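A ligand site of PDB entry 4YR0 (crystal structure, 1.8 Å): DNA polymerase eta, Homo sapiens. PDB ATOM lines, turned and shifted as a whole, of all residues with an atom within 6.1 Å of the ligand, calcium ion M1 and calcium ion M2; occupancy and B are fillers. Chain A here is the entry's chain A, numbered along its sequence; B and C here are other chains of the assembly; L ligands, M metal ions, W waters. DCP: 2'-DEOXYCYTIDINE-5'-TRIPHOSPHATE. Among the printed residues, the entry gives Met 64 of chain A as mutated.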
ATOM      1  N   ASP A  16      -7.759  12.595   0.734  1.00  0.00           N
ATOM      2  CA  ASP A  16      -8.349  12.721  -0.588  1.00  0.00           C
ATOM      3  C   ASP A  16      -7.535  11.944  -1.619  1.00  0.00           C
ATOM      4  O   ASP A  16      -6.334  12.171  -1.744  1.00  0.00           O
ATOM      5  CB  ASP A  16      -8.418  14.190  -1.005  1.00  0.00           C
ATOM      6  CG  ASP A  16      -8.780  14.345  -2.464  1.00  0.00           C
ATOM      7  OD1 ASP A  16      -9.963  14.251  -2.775  1.00  0.00           O
ATOM      8  OD2 ASP A  16      -7.885  14.541  -3.294  1.00  0.00           O
ATOM      9  N   MET A  17      -8.179  11.068  -2.373  1.00  0.00           N
ATOM     10  CA  MET A  17      -7.453  10.206  -3.316  1.00  0.00           C
ATOM     11  C   MET A  17      -6.902  11.025  -4.493  1.00  0.00           C
ATOM     12  O   MET A  17      -7.544  11.938  -4.982  1.00  0.00           O
ATOM     13  CB  MET A  17      -8.366   9.085  -3.841  1.00  0.00           C
ATOM     14  CG  MET A  17      -9.099   8.278  -2.752  1.00  0.00           C
ATOM     15  SD  MET A  17      -7.954   7.564  -1.533  1.00  0.00           S
ATOM     16  CE  MET A  17      -6.893   6.643  -2.591  1.00  0.00           C
ATOM     17  N   ASP A  18      -5.688  10.707  -4.924  1.00  0.00           N
ATOM     18  CA  ASP A  18      -5.120  11.404  -6.098  1.00  0.00           C
ATOM     19  C   ASP A  18      -5.819  10.946  -7.377  1.00  0.00           C
ATOM     20  O   ASP A  18      -6.034   9.740  -7.535  1.00  0.00           O
ATOM     21  CB  ASP A  18      -3.630  11.141  -6.218  1.00  0.00           C
ATOM     22  CG  ASP A  18      -2.850  11.665  -5.020  1.00  0.00           C
ATOM     23  OD1 ASP A  18      -3.258  12.676  -4.420  1.00  0.00           O
ATOM     24  OD2 ASP A  18      -1.818  11.067  -4.677  1.00  0.00           O
ATOM     25  N   CYS A  19      -6.160  11.905  -8.243  1.00  0.00           N
ATOM     26  CA  CYS A  19      -6.822  11.655  -9.549  1.00  0.00           C
ATOM     27  C   CYS A  19      -7.622  10.338  -9.539  1.00  0.00           C
ATOM     28  O   CYS A  19      -7.280   9.373 -10.235  1.00  0.00           O
ATOM     29  CB  CYS A  19      -5.792  11.670 -10.690  1.00  0.00           C
ATOM     30  SG  CYS A  19      -4.307  10.614 -10.552  1.00  0.00           S
ATOM     31  N   PHE A  20      -8.670  10.291  -8.726  1.00  0.00           N
ATOM     32  CA  PHE A  20      -9.209   9.009  -8.256  1.00  0.00           C
ATOM     33  C   PHE A  20      -9.681   8.053  -9.373  1.00  0.00           C
ATOM     34  O   PHE A  20      -9.241   6.914  -9.410  1.00  0.00           O
ATOM     35  CB  PHE A  20     -10.350   9.247  -7.254  1.00  0.00           C
ATOM     36  CG  PHE A  20     -10.876   7.972  -6.652  1.00  0.00           C
ATOM     37  CD1 PHE A  20     -10.009   7.012  -6.174  1.00  0.00           C
ATOM     38  CD2 PHE A  20     -12.254   7.737  -6.586  1.00  0.00           C
ATOM     39  CE1 PHE A  20     -10.490   5.816  -5.623  1.00  0.00           C
ATOM     40  CE2 PHE A  20     -12.736   6.550  -6.030  1.00  0.00           C
ATOM     41  CZ  PHE A  20     -11.851   5.598  -5.561  1.00  0.00           C
ATOM     42  N   PHE A  21     -10.560   8.495 -10.271  1.00  0.00           N
ATOM     43  CA  PHE A  21     -11.104   7.555 -11.267  1.00  0.00           C
ATOM     44  C   PHE A  21      -9.979   7.065 -12.173  1.00  0.00           C
ATOM     45  O   PHE A  21      -9.992   5.939 -12.636  1.00  0.00           O
ATOM     46  CB  PHE A  21     -12.220   8.168 -12.123  1.00  0.00           C
ATOM     47  CG  PHE A  21     -13.522   8.398 -11.388  1.00  0.00           C
ATOM     48  CD1 PHE A  21     -13.600   8.349 -10.010  1.00  0.00           C
ATOM     49  CD2 PHE A  21     -14.670   8.678 -12.107  1.00  0.00           C
ATOM     50  CE1 PHE A  21     -14.818   8.579  -9.347  1.00  0.00           C
ATOM     51  CE2 PHE A  21     -15.896   8.902 -11.454  1.00  0.00           C
ATOM     52  CZ  PHE A  21     -15.947   8.860 -10.081  1.00  0.00           C
ATOM     53  N   VAL A  22      -8.991   7.920 -12.432  1.00  0.00           N
ATOM     54  CA  VAL A  22      -7.818   7.509 -13.197  1.00  0.00           C
ATOM     55  C   VAL A  22      -7.046   6.382 -12.480  1.00  0.00           C
ATOM     56  O   VAL A  22      -6.685   5.368 -13.101  1.00  0.00           O
ATOM     57  CB  VAL A  22      -6.892   8.702 -13.479  1.00  0.00           C
ATOM     58  CG1 VAL A  22      -5.512   8.219 -13.923  1.00  0.00           C
ATOM     59  CG2 VAL A  22      -7.528   9.614 -14.548  1.00  0.00           C
ATOM     60  N   ILE A  51     -13.665  13.452 -17.196  1.00  0.00           N
ATOM     61  CA  ILE A  51     -14.057  13.710 -15.811  1.00  0.00           C
ATOM     62  C   ILE A  51     -12.958  13.448 -14.791  1.00  0.00           C
ATOM     63  O   ILE A  51     -13.153  13.731 -13.597  1.00  0.00           O
ATOM     64  CB  ILE A  51     -15.303  12.887 -15.418  1.00  0.00           C
ATOM     65  CG1 ILE A  51     -15.037  11.387 -15.499  1.00  0.00           C
ATOM     66  CG2 ILE A  51     -16.486  13.272 -16.312  1.00  0.00           C
ATOM     67  CD1 ILE A  51     -16.165  10.574 -14.868  1.00  0.00           C
ATOM     68  N   ALA A  52     -11.811  12.939 -15.244  1.00  0.00           N
ATOM     69  CA  ALA A  52     -10.615  12.806 -14.375  1.00  0.00           C
ATOM     70  C   ALA A  52      -9.328  12.720 -15.196  1.00  0.00           C
ATOM     71  O   ALA A  52      -9.323  12.153 -16.283  1.00  0.00           O
ATOM     72  CB  ALA A  52     -10.751  11.570 -13.467  1.00  0.00           C
ATOM     73  N   VAL A  53      -8.233  13.255 -14.656  1.00  0.00           N
ATOM     74  CA  VAL A  53      -6.997  13.460 -15.429  1.00  0.00           C
ATOM     75  C   VAL A  53      -5.765  13.083 -14.625  1.00  0.00           C
ATOM     76  O   VAL A  53      -5.607  13.566 -13.490  1.00  0.00           O
ATOM     77  CB  VAL A  53      -6.862  14.951 -15.874  1.00  0.00           C
ATOM     78  CG1 VAL A  53      -5.710  15.154 -16.839  1.00  0.00           C
ATOM     79  CG2 VAL A  53      -8.154  15.444 -16.469  1.00  0.00           C
ATOM     80  N   TYR A  55      -1.838  13.099 -13.430  1.00  0.00           N
ATOM     81  CA  TYR A  55      -0.948  14.238 -13.271  1.00  0.00           C
ATOM     82  C   TYR A  55      -0.034  14.404 -14.477  1.00  0.00           C
ATOM     83  O   TYR A  55       0.266  15.533 -14.844  1.00  0.00           O
ATOM     84  CB  TYR A  55      -0.153  14.113 -11.964  1.00  0.00           C
ATOM     85  CG  TYR A  55      -1.022  14.556 -10.798  1.00  0.00           C
ATOM     86  CD1 TYR A  55      -1.989  13.712 -10.268  1.00  0.00           C
ATOM     87  CD2 TYR A  55      -0.933  15.841 -10.302  1.00  0.00           C
ATOM     88  CE1 TYR A  55      -2.827  14.134  -9.258  1.00  0.00           C
ATOM     89  CE2 TYR A  55      -1.760  16.282  -9.283  1.00  0.00           C
ATOM     90  CZ  TYR A  55      -2.697  15.408  -8.756  1.00  0.00           C
ATOM     91  OH  TYR A  55      -3.515  15.847  -7.733  1.00  0.00           O
ATOM     92  N   ARG A  58      -2.058  16.384 -16.918  1.00  0.00           N
ATOM     93  CA  ARG A  58      -2.258  17.772 -16.485  1.00  0.00           C
ATOM     94  C   ARG A  58      -1.103  18.669 -16.914  1.00  0.00           C
ATOM     95  O   ARG A  58      -1.293  19.862 -17.153  1.00  0.00           O
ATOM     96  CB  ARG A  58      -2.433  17.880 -14.964  1.00  0.00           C
ATOM     97  CG  ARG A  58      -3.644  17.146 -14.447  1.00  0.00           C
ATOM     98  CD  ARG A  58      -3.745  17.197 -12.917  1.00  0.00           C
ATOM     99  NE  ARG A  58      -4.678  16.176 -12.460  1.00  0.00           N
ATOM    100  CZ  ARG A  58      -5.253  16.151 -11.268  1.00  0.00           C
ATOM    101  NH1 ARG A  58      -4.998  17.109 -10.374  1.00  0.00           N
ATOM    102  NH2 ARG A  58      -6.100  15.173 -10.978  1.00  0.00           N
ATOM    103  N   MET A  64     -10.327  18.584 -16.304  1.00  0.00           N
ATOM    104  CA  MET A  64     -11.720  18.172 -16.199  1.00  0.00           C
ATOM    105  C   MET A  64     -12.625  19.041 -17.082  1.00  0.00           C
ATOM    106  O   MET A  64     -12.299  20.186 -17.361  1.00  0.00           O
ATOM    107  CB  MET A  64     -12.207  18.285 -14.763  1.00  0.00           C
ATOM    108  CG  MET A  64     -12.092  17.015 -13.952  1.00  0.00           C
ATOM    109  SD  MET A  64     -12.556  17.408 -12.263  1.00  0.00           S
ATOM    110  CE  MET A  64     -11.738  16.053 -11.403  1.00  0.00           C
ATOM    111  N   SER A  65     -13.758  18.484 -17.492  1.00  0.00           N
ATOM    112  CA  SER A  65     -14.778  19.210 -18.263  1.00  0.00           C
ATOM    113  C   SER A  65     -14.233  19.733 -19.579  1.00  0.00           C
ATOM    114  O   SER A  65     -14.566  20.822 -20.030  1.00  0.00           O
ATOM    115  CB  SER A  65     -15.344  20.358 -17.434  1.00  0.00           C
ATOM    116  OG  SER A  65     -15.758  19.898 -16.166  1.00  0.00           O
ATOM    117  N   SER A 116     -17.164  12.733   0.052  1.00  0.00           N
ATOM    118  CA  SER A 116     -17.399  12.554  -1.377  1.00  0.00           C
ATOM    119  C   SER A 116     -17.027  11.139  -1.754  1.00  0.00           C
ATOM    120  O   SER A 116     -16.660  10.355  -0.905  1.00  0.00           O
ATOM    121  CB  SER A 116     -16.572  13.534  -2.219  1.00  0.00           C
ATOM    122  OG  SER A 116     -15.186  13.151  -2.259  1.00  0.00           O
ATOM    123  N   ILE A 117     -17.082  10.812  -3.041  1.00  0.00           N
ATOM    124  CA  ILE A 117     -16.719   9.483  -3.473  1.00  0.00           C
ATOM    125  C   ILE A 117     -15.239   9.164  -3.162  1.00  0.00           C
ATOM    126  O   ILE A 117     -14.895   7.997  -2.983  1.00  0.00           O
ATOM    127  CB  ILE A 117     -16.994   9.285  -4.989  1.00  0.00           C
ATOM    128  CG1 ILE A 117     -17.033   7.807  -5.356  1.00  0.00           C
ATOM    129  CG2 ILE A 117     -15.963   9.989  -5.833  1.00  0.00           C
ATOM    130  CD1 ILE A 117     -17.676   7.562  -6.717  1.00  0.00           C
ATOM    131  N   ASP A 118     -14.382  10.177  -3.039  1.00  0.00           N
ATOM    132  CA  ASP A 118     -12.952   9.882  -2.861  1.00  0.00           C
ATOM    133  C   ASP A 118     -12.286  10.605  -1.688  1.00  0.00           C
ATOM    134  O   ASP A 118     -11.056  10.701  -1.618  1.00  0.00           O
ATOM    135  CB  ASP A 118     -12.178  10.189  -4.156  1.00  0.00           C
ATOM    136  CG  ASP A 118     -11.738  11.642  -4.255  1.00  0.00           C
ATOM    137  OD1 ASP A 118     -12.478  12.566  -3.828  1.00  0.00           O
ATOM    138  OD2 ASP A 118     -10.615  11.856  -4.765  1.00  0.00           O
ATOM    139  N   GLU A 119     -13.082  11.104  -0.747  1.00  0.00           N
ATOM    140  CA  GLU A 119     -12.462  11.714   0.421  1.00  0.00           C
ATOM    141  C   GLU A 119     -13.303  11.591   1.683  1.00  0.00           C
ATOM    142  O   GLU A 119     -14.523  11.464   1.626  1.00  0.00           O
ATOM    143  CB  GLU A 119     -12.144  13.164   0.160  1.00  0.00           C
ATOM    144  CG  GLU A 119     -13.310  14.101   0.327  1.00  0.00           C
ATOM    145  CD  GLU A 119     -13.112  15.375  -0.464  1.00  0.00           C
ATOM    146  OE1 GLU A 119     -13.228  15.298  -1.700  1.00  0.00           O
ATOM    147  OE2 GLU A 119     -12.846  16.435   0.126  1.00  0.00           O
ATOM    148  N   LYS A 227      -8.921  20.434   4.848  1.00  0.00           N
ATOM    149  CA  LYS A 227      -9.201  20.399   3.414  1.00  0.00           C
ATOM    150  C   LYS A 227      -8.251  21.322   2.643  1.00  0.00           C
ATOM    151  O   LYS A 227      -7.663  20.925   1.636  1.00  0.00           O
ATOM    152  CB  LYS A 227     -10.662  20.782   3.138  1.00  0.00           C
ATOM    153  CG  LYS A 227     -11.048  20.867   1.650  1.00  0.00           C
ATOM    154  CD  LYS A 227     -10.937  19.511   0.962  1.00  0.00           C
ATOM    155  CE  LYS A 227     -11.438  19.571  -0.495  1.00  0.00           C
ATOM    156  NZ  LYS A 227     -11.132  18.286  -1.194  1.00  0.00           N
ATOM    157  N   LYS A 234       0.080  18.254  -3.466  1.00  0.00           N
ATOM    158  CA  LYS A 234      -0.473  17.044  -4.056  1.00  0.00           C
ATOM    159  C   LYS A 234       0.305  16.851  -5.336  1.00  0.00           C
ATOM    160  O   LYS A 234       0.824  17.816  -5.882  1.00  0.00           O
ATOM    161  CB  LYS A 234      -1.997  17.192  -4.271  1.00  0.00           C
ATOM    162  CG  LYS A 234      -2.409  18.238  -5.294  1.00  0.00           C
ATOM    163  CD  LYS A 234      -3.931  18.290  -5.423  1.00  0.00           C
ATOM    164  CE  LYS A 234      -4.376  19.006  -6.700  1.00  0.00           C
ATOM    165  NZ  LYS A 234      -5.871  19.048  -6.775  1.00  0.00           N
ATOM    166  N   PRO A 235       0.441  15.603  -5.805  1.00  0.00           N
ATOM    167  CA  PRO A 235      -0.148  14.380  -5.236  1.00  0.00           C
ATOM    168  C   PRO A 235       0.778  13.643  -4.291  1.00  0.00           C
ATOM    169  O   PRO A 235       1.943  14.005  -4.159  1.00  0.00           O
ATOM    170  CB  PRO A 235      -0.425  13.537  -6.477  1.00  0.00           C
ATOM    171  CG  PRO A 235       0.712  13.888  -7.393  1.00  0.00           C
ATOM    172  CD  PRO A 235       1.042  15.352  -7.124  1.00  0.00           C
ATOM    173  P    DT B   8     -15.241  19.688  -1.803  1.00  0.00           P
ATOM    174  OP1  DT B   8     -15.093  19.035  -0.481  1.00  0.00           O
ATOM    175  OP2  DT B   8     -14.334  20.778  -2.224  1.00  0.00           O
ATOM    176  O5'  DT B   8     -15.230  18.590  -2.956  1.00  0.00           O
ATOM    177  C5'  DT B   8     -15.972  17.394  -2.808  1.00  0.00           C
ATOM    178  C4'  DT B   8     -15.948  16.561  -4.091  1.00  0.00           C
ATOM    179  O4'  DT B   8     -17.017  16.954  -4.957  1.00  0.00           O
ATOM    180  C3'  DT B   8     -14.670  16.666  -4.943  1.00  0.00           C
ATOM    181  O3'  DT B   8     -13.997  15.422  -4.942  1.00  0.00           O
ATOM    182  C2'  DT B   8     -15.184  17.005  -6.363  1.00  0.00           C
ATOM    183  C1'  DT B   8     -16.649  16.605  -6.270  1.00  0.00           C
ATOM    184  N1   DT B   8     -17.532  17.315  -7.220  1.00  0.00           N
ATOM    185  C2   DT B   8     -18.449  16.589  -7.961  1.00  0.00           C
ATOM    186  O2   DT B   8     -18.576  15.381  -7.870  1.00  0.00           O
ATOM    187  N3   DT B   8     -19.215  17.342  -8.809  1.00  0.00           N
ATOM    188  C4   DT B   8     -19.150  18.698  -9.002  1.00  0.00           C
ATOM    189  O4   DT B   8     -19.888  19.285  -9.801  1.00  0.00           O
ATOM    190  C5   DT B   8     -18.175  19.406  -8.206  1.00  0.00           C
ATOM    191  C7   DT B   8     -18.013  20.888  -8.332  1.00  0.00           C
ATOM    192  C6   DT B   8     -17.419  18.684  -7.369  1.00  0.00           C
ATOM    193  P   8OG C   4     -24.073  17.805 -20.919  1.00  0.00           P
ATOM    194  OP1 8OG C   4     -25.539  17.477 -20.771  1.00  0.00           O
ATOM    195  OP2 8OG C   4     -23.518  19.163 -20.576  1.00  0.00           O
ATOM    196  O5' 8OG C   4     -23.276  16.749 -19.998  1.00  0.00           O
ATOM    197  C5' 8OG C   4     -22.940  15.447 -20.456  1.00  0.00           C
ATOM    198  C4' 8OG C   4     -22.852  14.513 -19.252  1.00  0.00           C
ATOM    199  O4' 8OG C   4     -21.941  15.041 -18.280  1.00  0.00           O
ATOM    200  C3' 8OG C   4     -24.184  14.351 -18.542  1.00  0.00           C
ATOM    201  O3' 8OG C   4     -24.220  12.952 -18.246  1.00  0.00           O
ATOM    202  C2' 8OG C   4     -24.048  15.141 -17.253  1.00  0.00           C
ATOM    203  C1' 8OG C   4     -22.560  14.992 -16.991  1.00  0.00           C
ATOM    204  N9  8OG C   4     -21.917  16.024 -16.144  1.00  0.00           N
ATOM    205  C8  8OG C   4     -22.053  17.355 -16.077  1.00  0.00           C
ATOM    206  N7  8OG C   4     -21.265  17.981 -15.200  1.00  0.00           N
ATOM    207  C5  8OG C   4     -20.544  17.001 -14.651  1.00  0.00           C
ATOM    208  C6  8OG C   4     -19.479  16.902 -13.628  1.00  0.00           C
ATOM    209  O6  8OG C   4     -19.077  17.947 -13.042  1.00  0.00           O
ATOM    210  N1  8OG C   4     -18.984  15.673 -13.347  1.00  0.00           N
ATOM    211  C2  8OG C   4     -19.424  14.555 -13.959  1.00  0.00           C
ATOM    212  N2  8OG C   4     -18.889  13.340 -13.639  1.00  0.00           N
ATOM    213  N3  8OG C   4     -20.382  14.571 -14.914  1.00  0.00           N
ATOM    214  C4  8OG C   4     -20.962  15.728 -15.282  1.00  0.00           C
ATOM    215  O8  8OG C   4     -22.904  17.994 -16.812  1.00  0.00           O
ATOM    216  P    DA C   5     -25.513  12.269 -17.571  1.00  0.00           P
ATOM    217  OP1  DA C   5     -25.780  11.094 -18.384  1.00  0.00           O
ATOM    218  OP2  DA C   5     -26.565  13.278 -17.326  1.00  0.00           O
ATOM    219  O5'  DA C   5     -24.966  11.850 -16.118  1.00  0.00           O
ATOM    220  C5'  DA C   5     -23.906  10.908 -15.999  1.00  0.00           C
ATOM    221  C4'  DA C   5     -23.611  10.610 -14.540  1.00  0.00           C
ATOM    222  O4'  DA C   5     -22.894  11.723 -13.955  1.00  0.00           O
ATOM    223  C3'  DA C   5     -24.839  10.383 -13.662  1.00  0.00           C
ATOM    224  O3'  DA C   5     -24.519   9.436 -12.641  1.00  0.00           O
ATOM    225  C2'  DA C   5     -25.067  11.777 -13.085  1.00  0.00           C
ATOM    226  C1'  DA C   5     -23.619  12.182 -12.836  1.00  0.00           C
ATOM    227  N9   DA C   5     -23.418  13.625 -12.704  1.00  0.00           N
ATOM    228  C8   DA C   5     -24.105  14.618 -13.335  1.00  0.00           C
ATOM    229  N7   DA C   5     -23.706  15.826 -13.002  1.00  0.00           N
ATOM    230  C5   DA C   5     -22.680  15.603 -12.090  1.00  0.00           C
ATOM    231  C6   DA C   5     -21.855  16.487 -11.347  1.00  0.00           C
ATOM    232  N6   DA C   5     -21.921  17.815 -11.437  1.00  0.00           N
ATOM    233  N1   DA C   5     -20.937  15.933 -10.526  1.00  0.00           N
ATOM    234  C2   DA C   5     -20.871  14.606 -10.437  1.00  0.00           C
ATOM    235  N3   DA C   5     -21.601  13.683 -11.070  1.00  0.00           N
ATOM    236  C4   DA C   5     -22.494  14.261 -11.884  1.00  0.00           C
HETATM  237  N1  DCP L   1     -15.492  13.894 -10.236  1.00  0.00           N
HETATM  238  C2  DCP L   1     -16.558  14.065 -11.116  1.00  0.00           C
HETATM  239  N3  DCP L   1     -16.993  15.305 -11.418  1.00  0.00           N
HETATM  240  C4  DCP L   1     -16.385  16.398 -10.896  1.00  0.00           C
HETATM  241  C5  DCP L   1     -15.310  16.247 -10.025  1.00  0.00           C
HETATM  242  C6  DCP L   1     -14.874  14.957  -9.703  1.00  0.00           C
HETATM  243  O2  DCP L   1     -17.108  13.054 -11.604  1.00  0.00           O
HETATM  244  N4  DCP L   1     -16.830  17.632 -11.225  1.00  0.00           N
HETATM  245  C1' DCP L   1     -15.039  12.541  -9.909  1.00  0.00           C
HETATM  246  C2' DCP L   1     -13.801  12.231 -10.753  1.00  0.00           C
HETATM  247  C3' DCP L   1     -12.644  12.354  -9.766  1.00  0.00           C
HETATM  248  C4' DCP L   1     -13.274  12.080  -8.402  1.00  0.00           C
HETATM  249  O4' DCP L   1     -14.636  12.514  -8.538  1.00  0.00           O
HETATM  250  O3' DCP L   1     -11.569  11.457 -10.096  1.00  0.00           O
HETATM  251  C5' DCP L   1     -12.626  12.857  -7.258  1.00  0.00           C
HETATM  252  O5' DCP L   1     -12.640  14.226  -7.627  1.00  0.00           O
HETATM  253  PA  DCP L   1     -11.525  15.242  -7.158  1.00  0.00           P
HETATM  254  O1A DCP L   1     -12.149  16.612  -7.331  1.00  0.00           O
HETATM  255  O2A DCP L   1     -11.011  14.852  -5.807  1.00  0.00           O
HETATM  256  O3A DCP L   1     -10.400  15.134  -8.315  1.00  0.00           O
HETATM  257  PB  DCP L   1      -9.336  13.952  -8.573  1.00  0.00           P
HETATM  258  O1B DCP L   1      -9.622  13.381  -9.941  1.00  0.00           O
HETATM  259  O2B DCP L   1      -9.308  12.931  -7.467  1.00  0.00           O
HETATM  260  O3B DCP L   1      -7.944  14.759  -8.701  1.00  0.00           O
HETATM  261  PG  DCP L   1      -7.084  15.397  -7.473  1.00  0.00           P
HETATM  262  O1G DCP L   1      -6.830  16.817  -7.934  1.00  0.00           O
HETATM  263  O2G DCP L   1      -5.815  14.559  -7.445  1.00  0.00           O
HETATM  264  O3G DCP L   1      -7.954  15.301  -6.254  1.00  0.00           O
HETATM  265 CA    CA M   1      -9.096  13.583  -5.241  1.00  0.00          CA
HETATM  266 CA    CA M   2     -12.027  14.895  -3.634  1.00  0.00          CA
HETATM  267  O   HOH W   1      -8.779  14.553 -12.310  1.00  0.00           O
HETATM  268  O   HOH W   2     -10.865  18.671  -8.949  1.00  0.00           O
HETATM  269  O   HOH W   3     -11.492  17.138  -3.988  1.00  0.00           O
HETATM  270  O   HOH W   4     -15.006  19.859 -10.421  1.00  0.00           O
HETATM  271  O   HOH W   5      -8.326  18.287  -9.517  1.00  0.00           O
HETATM  272  O   HOH W   6     -15.599  13.428  -6.003  1.00  0.00           O
HETATM  273  O   HOH W   7      -5.563  14.291  -4.026  1.00  0.00           O
HETATM  274  O   HOH W   8      -8.820  17.624  -5.201  1.00  0.00           O
HETATM  275  O   HOH W   9     -18.558  10.804 -11.420  1.00  0.00           O
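The side-chain amino group (NZ) of Lys 227 is in salt-bridge range of the side-chain carboxylate (OE2) of Glu 119 (2.8 Å). The backbone NH (N) of Glu 119 is in hydrogen-bond range of the side-chain hydroxyl (OG) of Ser 116 (3.3 Å). The guanidinium group (NE) of Arg 58 lies within hydrogen-bond range of the backbone carbonyl oxygen (O) of Val 53 (3.0 Å). The side-chain hydroxyl (OH) of Tyr 55 sits at hydrogen-bond distance from the guanidinium group (NH1) of Arg 58, 3.3 Å away. N of Asp 118 lies close to OG of Ser 116.
Merely in contact with the ligand: Ile 51, Ala 52, Met 64, Asp 18 and Ile 117. Hydrophobic or aromatic side chains that line the ligand: Phe 20, Phe 21, Ala 52, Tyr 55, Met 64 and Ile 117. 16 residues have an atom within 4 Å of the ligand: Asp 16, Met 17, Asp 18, Cys 19, Phe 20, Phe 21, Ile 51, Ala 52, Tyr 55, Arg 58, Met 64, Ile 117, Asp 118, Lys 234, DT 8 of chain B and 8OG 4 of chain C.
Calcium ion M2 is bound by the side-chain carboxylate of Glu 119 (2.3 Å), the side-chain carboxylate of Asp 16 (2.3 Å), water W3 (2.3 Å), the side-chain carboxylate of Asp 118 (2.4 Å), an oxygen (O2A) of the ligand (2.4 Å) and O3' of DT 8 of chain B (2.4 Å). Calcium ion M2 has six donor atoms within binding distance.
Calcium ion M1 is bound by O of Met 17, O3G of the ligand, O2B of the ligand, OD2 of Asp 118, O2A of the ligand, OD2 of Asp 16 and OD1 of Asp 16.
Water W3 lies within hydrogen-bond range of the side-chain amino group of Lys 227 (3.0 Å) and an oxygen (O1A) of the ligand (3.4 Å). Water W9 bridges an oxygen (O2) of the ligand (2.7 Å) and N2 of 8OG 4 of chain C (3.4 Å). Water W1 lies within hydrogen-bond range of N of Val 53, O1B of the ligand and NH2 of Arg 58. Water W7 lies within hydrogen-bond range of the side-chain carboxylate (OD1) of Asp 18, the backbone carbonyl oxygen (O) of Asp 16 and an oxygen (O2G) of the ligand.
Within 4 Å of calcium ion M1: Asp 16, Met 17 and Asp 118.
OG of Ser 116 touches calcium ion M2, 3.9 Å away. The nearest printed residue that does not touch calcium ion M2 is Lys 227 (4.3 Å).
N3 of DT 8 of chain B lies close to a nitrogen (N4) of the ligand (3.4 Å). NH1 of Arg 58 lies within salt-bridge range of O1G of the ligand (3.1 Å). O3' of the ligand is in hydrogen-bond range of N of Phe 21 (3.1 Å). OH of Tyr 55 is in hydrogen-bond range of O2G of the ligand, at 2.7 Å. The side-chain amino group (NZ) of Lys 234 lies within salt-bridge range of an oxygen (O1G) of the ligand, at 2.7 Å. O6 of 8OG 4 of chain C is in hydrogen-bond range of N4 of the ligand, 2.9 Å away. The backbone NH (N) of Phe 20 is in hydrogen-bond range of an oxygen (O3') of the ligand (3.4 Å). The backbone NH of Cys 19 is in hydrogen-bond range of an oxygen (O2G) of the ligand, at 2.8 Å.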
